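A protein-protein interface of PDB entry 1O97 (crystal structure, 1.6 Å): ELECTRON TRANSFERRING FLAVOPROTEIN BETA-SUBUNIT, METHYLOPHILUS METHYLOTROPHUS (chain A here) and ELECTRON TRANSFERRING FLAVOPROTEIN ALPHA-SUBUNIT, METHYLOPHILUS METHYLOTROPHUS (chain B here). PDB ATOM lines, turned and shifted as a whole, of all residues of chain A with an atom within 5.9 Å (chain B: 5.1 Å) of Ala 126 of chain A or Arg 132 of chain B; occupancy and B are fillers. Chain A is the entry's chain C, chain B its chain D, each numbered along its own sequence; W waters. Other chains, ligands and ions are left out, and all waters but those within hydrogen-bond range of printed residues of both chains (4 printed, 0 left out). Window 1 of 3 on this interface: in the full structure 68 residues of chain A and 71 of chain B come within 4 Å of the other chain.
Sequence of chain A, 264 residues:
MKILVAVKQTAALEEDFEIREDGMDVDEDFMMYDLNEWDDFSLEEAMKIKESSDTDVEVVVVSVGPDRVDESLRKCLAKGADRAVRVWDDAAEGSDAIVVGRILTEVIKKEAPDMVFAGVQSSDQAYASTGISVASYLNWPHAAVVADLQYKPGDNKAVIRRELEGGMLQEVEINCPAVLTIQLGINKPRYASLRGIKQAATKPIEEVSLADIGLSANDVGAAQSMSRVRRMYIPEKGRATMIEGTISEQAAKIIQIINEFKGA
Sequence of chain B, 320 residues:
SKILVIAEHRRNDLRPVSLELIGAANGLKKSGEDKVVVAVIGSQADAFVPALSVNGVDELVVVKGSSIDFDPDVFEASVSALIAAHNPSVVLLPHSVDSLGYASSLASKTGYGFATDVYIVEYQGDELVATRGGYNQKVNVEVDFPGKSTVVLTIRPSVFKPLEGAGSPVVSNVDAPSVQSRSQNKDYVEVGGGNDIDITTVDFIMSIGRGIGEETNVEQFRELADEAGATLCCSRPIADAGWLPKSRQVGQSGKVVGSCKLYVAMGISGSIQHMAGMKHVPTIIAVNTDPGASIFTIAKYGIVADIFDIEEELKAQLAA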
ATOM      1  N   GLN A 121      -2.518  23.877  -3.608  1.00  0.00           N
ATOM      2  CA  GLN A 121      -2.069  23.915  -5.031  1.00  0.00           C
ATOM      3  C   GLN A 121      -3.275  24.128  -5.925  1.00  0.00           C
ATOM      4  O   GLN A 121      -4.419  24.105  -5.452  1.00  0.00           O
ATOM      5  CB  GLN A 121      -1.424  22.589  -5.393  1.00  0.00           C
ATOM      6  CG  GLN A 121      -2.361  21.381  -5.402  1.00  0.00           C
ATOM      7  CD  GLN A 121      -1.604  20.111  -5.790  1.00  0.00           C
ATOM      8  OE1 GLN A 121      -2.108  19.321  -6.586  1.00  0.00           O
ATOM      9  NE2 GLN A 121      -0.414  19.920  -5.239  1.00  0.00           N
ATOM     10  N   SER A 122      -2.965  24.359  -7.206  1.00  0.00           N
ATOM     11  CA  SER A 122      -4.048  24.493  -8.234  1.00  0.00           C
ATOM     12  C   SER A 122      -4.250  23.143  -8.889  1.00  0.00           C
ATOM     13  O   SER A 122      -3.320  22.364  -9.065  1.00  0.00           O
ATOM     14  CB  SER A 122      -3.647  25.573  -9.248  1.00  0.00           C
ATOM     15  OG  SER A 122      -2.353  25.323  -9.762  1.00  0.00           O
ATOM     16  N   SER A 123      -5.504  22.863  -9.227  1.00  0.00           N
ATOM     17  CA  SER A 123      -5.821  21.577  -9.872  1.00  0.00           C
ATOM     18  C   SER A 123      -5.309  21.507 -11.289  1.00  0.00           C
ATOM     19  O   SER A 123      -5.095  20.391 -11.765  1.00  0.00           O
ATOM     20  CB  SER A 123      -7.329  21.300  -9.855  1.00  0.00           C
ATOM     21  OG  SER A 123      -7.998  22.266 -10.566  1.00  0.00           O
ATOM     22  N   ASP A 124      -5.119  22.649 -11.931  1.00  0.00           N
ATOM     23  CA  ASP A 124      -4.566  22.613 -13.299  1.00  0.00           C
ATOM     24  C   ASP A 124      -3.065  22.404 -13.334  1.00  0.00           C
ATOM     25  O   ASP A 124      -2.597  21.357 -13.784  1.00  0.00           O
ATOM     26  CB  ASP A 124      -5.089  23.761 -14.209  1.00  0.00           C
ATOM     27  CG  ASP A 124      -5.023  25.147 -13.595  1.00  0.00           C
ATOM     28  OD1 ASP A 124      -4.332  25.378 -12.538  1.00  0.00           O
ATOM     29  OD2 ASP A 124      -5.602  26.109 -14.140  1.00  0.00           O
ATOM     30  N   GLN A 125      -2.316  23.408 -12.877  1.00  0.00           N
ATOM     31  CA  GLN A 125      -0.855  23.348 -12.958  1.00  0.00           C
ATOM     32  C   GLN A 125      -0.155  22.769 -11.728  1.00  0.00           C
ATOM     33  O   GLN A 125       0.985  22.296 -11.864  1.00  0.00           O
ATOM     34  CB  GLN A 125      -0.314  24.747 -13.253  1.00  0.00           C
ATOM     35  CG  GLN A 125      -0.974  25.416 -14.510  1.00  0.00           C
ATOM     36  CD  GLN A 125      -1.374  24.458 -15.706  1.00  0.00           C
ATOM     37  OE1 GLN A 125      -0.786  23.426 -15.969  1.00  0.00           O
ATOM     38  NE2 GLN A 125      -2.369  24.898 -16.452  1.00  0.00           N
ATOM     39  N   ALA A 126      -0.844  22.750 -10.579  1.00  0.00           N
ATOM     40  CA  ALA A 126      -0.272  22.121  -9.349  1.00  0.00           C
ATOM     41  C   ALA A 126       1.153  22.570  -9.115  1.00  0.00           C
ATOM     42  O   ALA A 126       2.037  21.710  -8.870  1.00  0.00           O
ATOM     43  CB  ALA A 126      -0.394  20.598  -9.409  1.00  0.00           C
ATOM     44  N   TYR A 127       1.358  23.887  -9.098  1.00  0.00           N
ATOM     45  CA  TYR A 127       2.678  24.458  -8.751  1.00  0.00           C
ATOM     46  C   TYR A 127       3.002  24.253  -7.275  1.00  0.00           C
ATOM     47  O   TYR A 127       4.154  23.999  -6.936  1.00  0.00           O
ATOM     48  CB  TYR A 127       2.785  25.948  -9.052  1.00  0.00           C
ATOM     49  CG  TYR A 127       2.579  26.286 -10.529  1.00  0.00           C
ATOM     50  CD1 TYR A 127       1.663  27.215 -10.906  1.00  0.00           C
ATOM     51  CD2 TYR A 127       3.349  25.680 -11.530  1.00  0.00           C
ATOM     52  CE1 TYR A 127       1.490  27.579 -12.241  1.00  0.00           C
ATOM     53  CE2 TYR A 127       3.150  26.007 -12.903  1.00  0.00           C
ATOM     54  CZ  TYR A 127       2.217  26.969 -13.239  1.00  0.00           C
ATOM     55  OH  TYR A 127       1.962  27.389 -14.575  1.00  0.00           O
ATOM     56  N   ALA A 128       1.965  24.377  -6.446  1.00  0.00           N
ATOM     57  CA  ALA A 128       2.113  24.366  -4.985  1.00  0.00           C
ATOM     58  C   ALA A 128       3.167  25.369  -4.588  1.00  0.00           C
ATOM     59  O   ALA A 128       4.055  25.056  -3.756  1.00  0.00           O
ATOM     60  CB  ALA A 128       2.451  22.944  -4.456  1.00  0.00           C
ATOM     61  N   HIS B  95       9.824  16.993  -3.690  1.00  0.00           N
ATOM     62  CA  HIS B  95       8.524  17.694  -3.746  1.00  0.00           C
ATOM     63  C   HIS B  95       7.646  17.035  -2.695  1.00  0.00           C
ATOM     64  O   HIS B  95       6.904  16.097  -3.000  1.00  0.00           O
ATOM     65  CB  HIS B  95       7.869  17.604  -5.136  1.00  0.00           C
ATOM     66  CG  HIS B  95       6.650  18.463  -5.274  1.00  0.00           C
ATOM     67  ND1 HIS B  95       6.735  19.835  -5.348  1.00  0.00           N
ATOM     68  CD2 HIS B  95       5.334  18.158  -5.372  1.00  0.00           C
ATOM     69  CE1 HIS B  95       5.523  20.349  -5.482  1.00  0.00           C
ATOM     70  NE2 HIS B  95       4.654  19.354  -5.470  1.00  0.00           N
ATOM     71  N   ALA B 115      11.469  25.406 -10.662  1.00  0.00           N
ATOM     72  CA  ALA B 115      10.294  24.617 -11.115  1.00  0.00           C
ATOM     73  C   ALA B 115       9.989  23.526 -10.128  1.00  0.00           C
ATOM     74  O   ALA B 115      10.910  23.051  -9.487  1.00  0.00           O
ATOM     75  CB  ALA B 115      10.540  24.000 -12.494  1.00  0.00           C
ATOM     76  N   THR B 116       8.710  23.194  -9.982  1.00  0.00           N
ATOM     77  CA  THR B 116       8.292  22.190  -8.993  1.00  0.00           C
ATOM     78  C   THR B 116       7.706  20.925  -9.588  1.00  0.00           C
ATOM     79  O   THR B 116       7.212  20.936 -10.741  1.00  0.00           O
ATOM     80  CB  THR B 116       7.211  22.737  -8.022  1.00  0.00           C
ATOM     81  OG1 THR B 116       6.039  23.092  -8.780  1.00  0.00           O
ATOM     82  CG2 THR B 116       7.690  23.990  -7.358  1.00  0.00           C
ATOM     83  N   ASP B 117       7.797  19.841  -8.811  1.00  0.00           N
ATOM     84  CA  ASP B 117       7.192  18.541  -9.116  1.00  0.00           C
ATOM     85  C   ASP B 117       7.703  18.026 -10.485  1.00  0.00           C
ATOM     86  O   ASP B 117       6.924  17.551 -11.335  1.00  0.00           O
ATOM     87  CB  ASP B 117       5.644  18.621  -9.036  1.00  0.00           C
ATOM     88  CG  ASP B 117       5.000  17.252  -8.971  1.00  0.00           C
ATOM     89  OD1 ASP B 117       5.645  16.276  -8.566  1.00  0.00           O
ATOM     90  OD2 ASP B 117       3.827  17.093  -9.318  1.00  0.00           O
ATOM     91  N   VAL B 118       9.007  18.152 -10.648  1.00  0.00           N
ATOM     92  CA  VAL B 118       9.697  17.752 -11.875  1.00  0.00           C
ATOM     93  C   VAL B 118       9.915  16.239 -11.929  1.00  0.00           C
ATOM     94  O   VAL B 118      10.342  15.604 -10.956  1.00  0.00           O
ATOM     95  CB  VAL B 118      11.025  18.540 -11.967  1.00  0.00           C
ATOM     96  CG1 VAL B 118      11.977  17.976 -13.051  1.00  0.00           C
ATOM     97  CG2 VAL B 118      10.746  19.981 -12.165  1.00  0.00           C
ATOM     98  N   TYR B 119       9.631  15.649 -13.097  1.00  0.00           N
ATOM     99  CA  TYR B 119       9.795  14.198 -13.284  1.00  0.00           C
ATOM    100  C   TYR B 119      10.669  13.791 -14.493  1.00  0.00           C
ATOM    101  O   TYR B 119      10.866  12.582 -14.735  1.00  0.00           O
ATOM    102  CB  TYR B 119       8.450  13.442 -13.268  1.00  0.00           C
ATOM    103  CG  TYR B 119       7.395  13.991 -14.183  1.00  0.00           C
ATOM    104  CD1 TYR B 119       7.367  13.645 -15.545  1.00  0.00           C
ATOM    105  CD2 TYR B 119       6.417  14.832 -13.683  1.00  0.00           C
ATOM    106  CE1 TYR B 119       6.386  14.108 -16.357  1.00  0.00           C
ATOM    107  CE2 TYR B 119       5.396  15.319 -14.486  1.00  0.00           C
ATOM    108  CZ  TYR B 119       5.385  14.976 -15.829  1.00  0.00           C
ATOM    109  OH  TYR B 119       4.340  15.426 -16.598  1.00  0.00           O
ATOM    110  N   ALA B 130      14.022  20.846 -17.794  1.00  0.00           N
ATOM    111  CA  ALA B 130      13.185  20.102 -16.832  1.00  0.00           C
ATOM    112  C   ALA B 130      11.753  19.940 -17.371  1.00  0.00           C
ATOM    113  O   ALA B 130      11.271  20.804 -18.066  1.00  0.00           O
ATOM    114  CB  ALA B 130      13.145  20.877 -15.454  1.00  0.00           C
ATOM    115  N   THR B 131      11.082  18.828 -17.052  1.00  0.00           N
ATOM    116  CA  THR B 131       9.709  18.600 -17.503  1.00  0.00           C
ATOM    117  C   THR B 131       8.834  18.333 -16.294  1.00  0.00           C
ATOM    118  O   THR B 131       9.218  17.540 -15.414  1.00  0.00           O
ATOM    119  CB  THR B 131       9.653  17.379 -18.442  1.00  0.00           C
ATOM    120  OG1 THR B 131      10.536  17.618 -19.559  1.00  0.00           O
ATOM    121  CG2 THR B 131       8.212  17.200 -19.060  1.00  0.00           C
ATOM    122  N   ARG B 132       7.683  18.970 -16.313  1.00  0.00           N
ATOM    123  CA  ARG B 132       6.676  18.737 -15.290  1.00  0.00           C
ATOM    124  C   ARG B 132       5.327  18.616 -15.949  1.00  0.00           C
ATOM    125  O   ARG B 132       5.243  18.623 -17.172  1.00  0.00           O
ATOM    126  CB  ARG B 132       6.687  19.907 -14.299  1.00  0.00           C
ATOM    127  CG  ARG B 132       6.157  21.226 -14.889  1.00  0.00           C
ATOM    128  CD  ARG B 132       6.214  22.506 -14.019  1.00  0.00           C
ATOM    129  NE  ARG B 132       5.772  22.222 -12.647  1.00  0.00           N
ATOM    130  CZ  ARG B 132       4.498  22.202 -12.261  1.00  0.00           C
ATOM    131  NH1 ARG B 132       3.517  22.464 -13.122  1.00  0.00           N
ATOM    132  NH2 ARG B 132       4.188  21.933 -10.992  1.00  0.00           N
ATOM    133  N   GLY B 133       4.280  18.390 -15.156  1.00  0.00           N
ATOM    134  CA  GLY B 133       2.933  18.210 -15.713  1.00  0.00           C
ATOM    135  C   GLY B 133       2.176  19.481 -15.929  1.00  0.00           C
ATOM    136  O   GLY B 133       2.510  20.589 -15.455  1.00  0.00           O
ATOM    137  N   GLY B 134       1.179  19.376 -16.802  1.00  0.00           N
ATOM    138  CA  GLY B 134       0.213  20.460 -16.930  1.00  0.00           C
ATOM    139  C   GLY B 134      -1.217  19.952 -17.061  1.00  0.00           C
ATOM    140  O   GLY B 134      -1.440  18.786 -17.468  1.00  0.00           O
ATOM    141  N   GLN B 137      -2.187  16.784 -15.285  1.00  0.00           N
ATOM    142  CA  GLN B 137      -1.306  15.735 -15.824  1.00  0.00           C
ATOM    143  C   GLN B 137      -1.730  15.235 -17.238  1.00  0.00           C
ATOM    144  O   GLN B 137      -1.322  14.119 -17.689  1.00  0.00           O
ATOM    145  CB  GLN B 137      -1.217  14.545 -14.860  1.00  0.00           C
ATOM    146  CG  GLN B 137      -0.277  14.789 -13.672  1.00  0.00           C
ATOM    147  CD  GLN B 137       1.131  15.160 -14.112  1.00  0.00           C
ATOM    148  OE1 GLN B 137       1.756  16.033 -13.523  1.00  0.00           O
ATOM    149  NE2 GLN B 137       1.624  14.508 -15.164  1.00  0.00           N
ATOM    150  N   VAL B 139      -0.902  17.033 -20.014  1.00  0.00           N
ATOM    151  CA  VAL B 139       0.242  17.330 -20.850  1.00  0.00           C
ATOM    152  C   VAL B 139       1.562  17.308 -20.071  1.00  0.00           C
ATOM    153  O   VAL B 139       1.588  17.287 -18.819  1.00  0.00           O
ATOM    154  CB  VAL B 139       0.132  18.705 -21.539  1.00  0.00           C
ATOM    155  CG1 VAL B 139      -1.150  18.828 -22.395  1.00  0.00           C
ATOM    156  CG2 VAL B 139       0.151  19.863 -20.512  1.00  0.00           C
ATOM    157  N   ASN B 140       2.675  17.280 -20.784  1.00  0.00           N
ATOM    158  CA  ASN B 140       4.002  17.595 -20.252  1.00  0.00           C
ATOM    159  C   ASN B 140       4.343  18.996 -20.662  1.00  0.00           C
ATOM    160  O   ASN B 140       4.059  19.444 -21.796  1.00  0.00           O
ATOM    161  CB  ASN B 140       5.108  16.671 -20.804  1.00  0.00           C
ATOM    162  CG  ASN B 140       5.142  15.324 -20.118  1.00  0.00           C
ATOM    163  OD1 ASN B 140       4.276  15.008 -19.317  1.00  0.00           O
ATOM    164  ND2 ASN B 140       6.136  14.498 -20.491  1.00  0.00           N
ATOM    165  N   VAL B 141       4.980  19.717 -19.722  1.00  0.00           N
ATOM    166  CA  VAL B 141       5.456  21.066 -19.948  1.00  0.00           C
ATOM    167  C   VAL B 141       6.963  21.046 -19.758  1.00  0.00           C
ATOM    168  O   VAL B 141       7.496  20.710 -18.699  1.00  0.00           O
ATOM    169  CB  VAL B 141       4.797  22.089 -18.949  1.00  0.00           C
ATOM    170  CG1 VAL B 141       5.192  23.517 -19.325  1.00  0.00           C
ATOM    171  CG2 VAL B 141       3.233  21.971 -18.958  1.00  0.00           C
HETATM  172  O   HOH W   1      -0.788  19.078 -13.976  1.00  0.00           O
HETATM  173  O   HOH W   2       1.644  19.696 -12.746  1.00  0.00           O
HETATM  174  O   HOH W   3       2.051  19.836  -6.612  1.00  0.00           O
HETATM  175  O   HOH W   4       2.462  19.128 -10.426  1.00  0.00           O
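Of the printed residues of chain B, Ala 126 of chain A touches Arg 132. Printed residues of chain A within 4 Å of Arg 132 of chain B: Gln 125, Ala 126 and Tyr 127. Printed residues of chain A within 4 Å of Thr 116 of chain B: Tyr 127. Of the printed residues of chain B, Tyr 127 of chain A touches Thr 116 and Arg 132. Printed residues of chain A within 4 Å of Gly 134 of chain B: Asp 124 and Gln 125. Asn 140 of chain B touches none of the printed residues of chain A. Ser 122 of chain A touches none of the printed residues of chain B. The nearest residue of chain B that does not touch Ala 126 of chain A is Thr 116 of chain B (4.2 Å). The nearest printed residue of chain B that does not touch Gln 125 of chain A is Gly 133 of chain B (4.3 Å).
Asp 124 of chain A touches Gly 134 of chain B (O to C, 3.8 Å). CA of Gly 134 of chain B touches OE1 of Gln 125 of chain A, 3.3 Å away. NH1 of Arg 132 of chain B touches CE2 of Tyr 127 of chain A (3.6 Å).
Of the 15 printed residues of chain B, 3 touch a printed residue of chain A. Printed residues of chain B that touch a printed residue of chain A: Thr 116, Arg 132 and Gly 134. Among the printed residues, 6 pairs touch across the chains.
OG of Ser 122 of chain A sits close to OD1 of Asp 124 of chain A. The backbone NH (N) of Ala 126 of chain A is in hydrogen-bond range of the side-chain hydroxyl (OG) of Ser 122 of chain A, at 3.1 Å. The backbone carbonyl oxygen (O) of Thr 116 of chain B is in hydrogen-bond range of the guanidinium group (NE) of Arg 132 of chain B (2.7 Å). The side-chain hydroxyl of Tyr 119 of chain B is in hydrogen-bond range of the backbone carbonyl oxygen of Arg 132 of chain B (3.4 Å). The backbone carbonyl oxygen (O) of Arg 132 of chain B lies within hydrogen-bond range of the backbone NH (N) of Val 141 of chain B. The backbone NH of Gly 134 of chain B sits at hydrogen-bond distance from the backbone carbonyl oxygen of Val 139 of chain B, 2.9 Å away.
Water W4 lies within hydrogen-bond range of the side-chain carboxylate (OD2) of Asp 117 of chain B, the backbone carbonyl oxygen (O) of Ala 126 of chain A and the guanidinium group (NH2) of Arg 132 of chain B. Water W3 lies within hydrogen-bond range of NE2 of Gln 121 of chain A (2.8 Å), NE2 of His 95 of chain B (2.9 Å) and O of Ala 126 of chain A (2.9 Å). Water W2 lies within hydrogen-bond range of O of Gln 125 of chain A, O of Gly 133 of chain B and NH1 of Arg 132 of chain B. Water W1 lies within hydrogen-bond range of the backbone carbonyl oxygen of Asp 124 of chain A (2.9 Å), the backbone NH of Gln 137 of chain B (3.0 Å) and the backbone NH of Gly 134 of chain B (3.5 Å).
The guanidinium group (NH1) of Arg 132 of chain B lies within hydrogen-bond range of the backbone carbonyl oxygen (O) of Gln 125 of chain A, 2.8 Å away. The backbone carbonyl oxygen (O) of Ala 126 of chain A sits at hydrogen-bond distance from the guanidinium group (NH2) of Arg 132 of chain B (3.0 Å). The backbone carbonyl oxygen (O) of Tyr 127 of chain A lies within hydrogen-bond range of the side-chain hydroxyl (OG1) of Thr 116 of chain B (2.8 Å).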
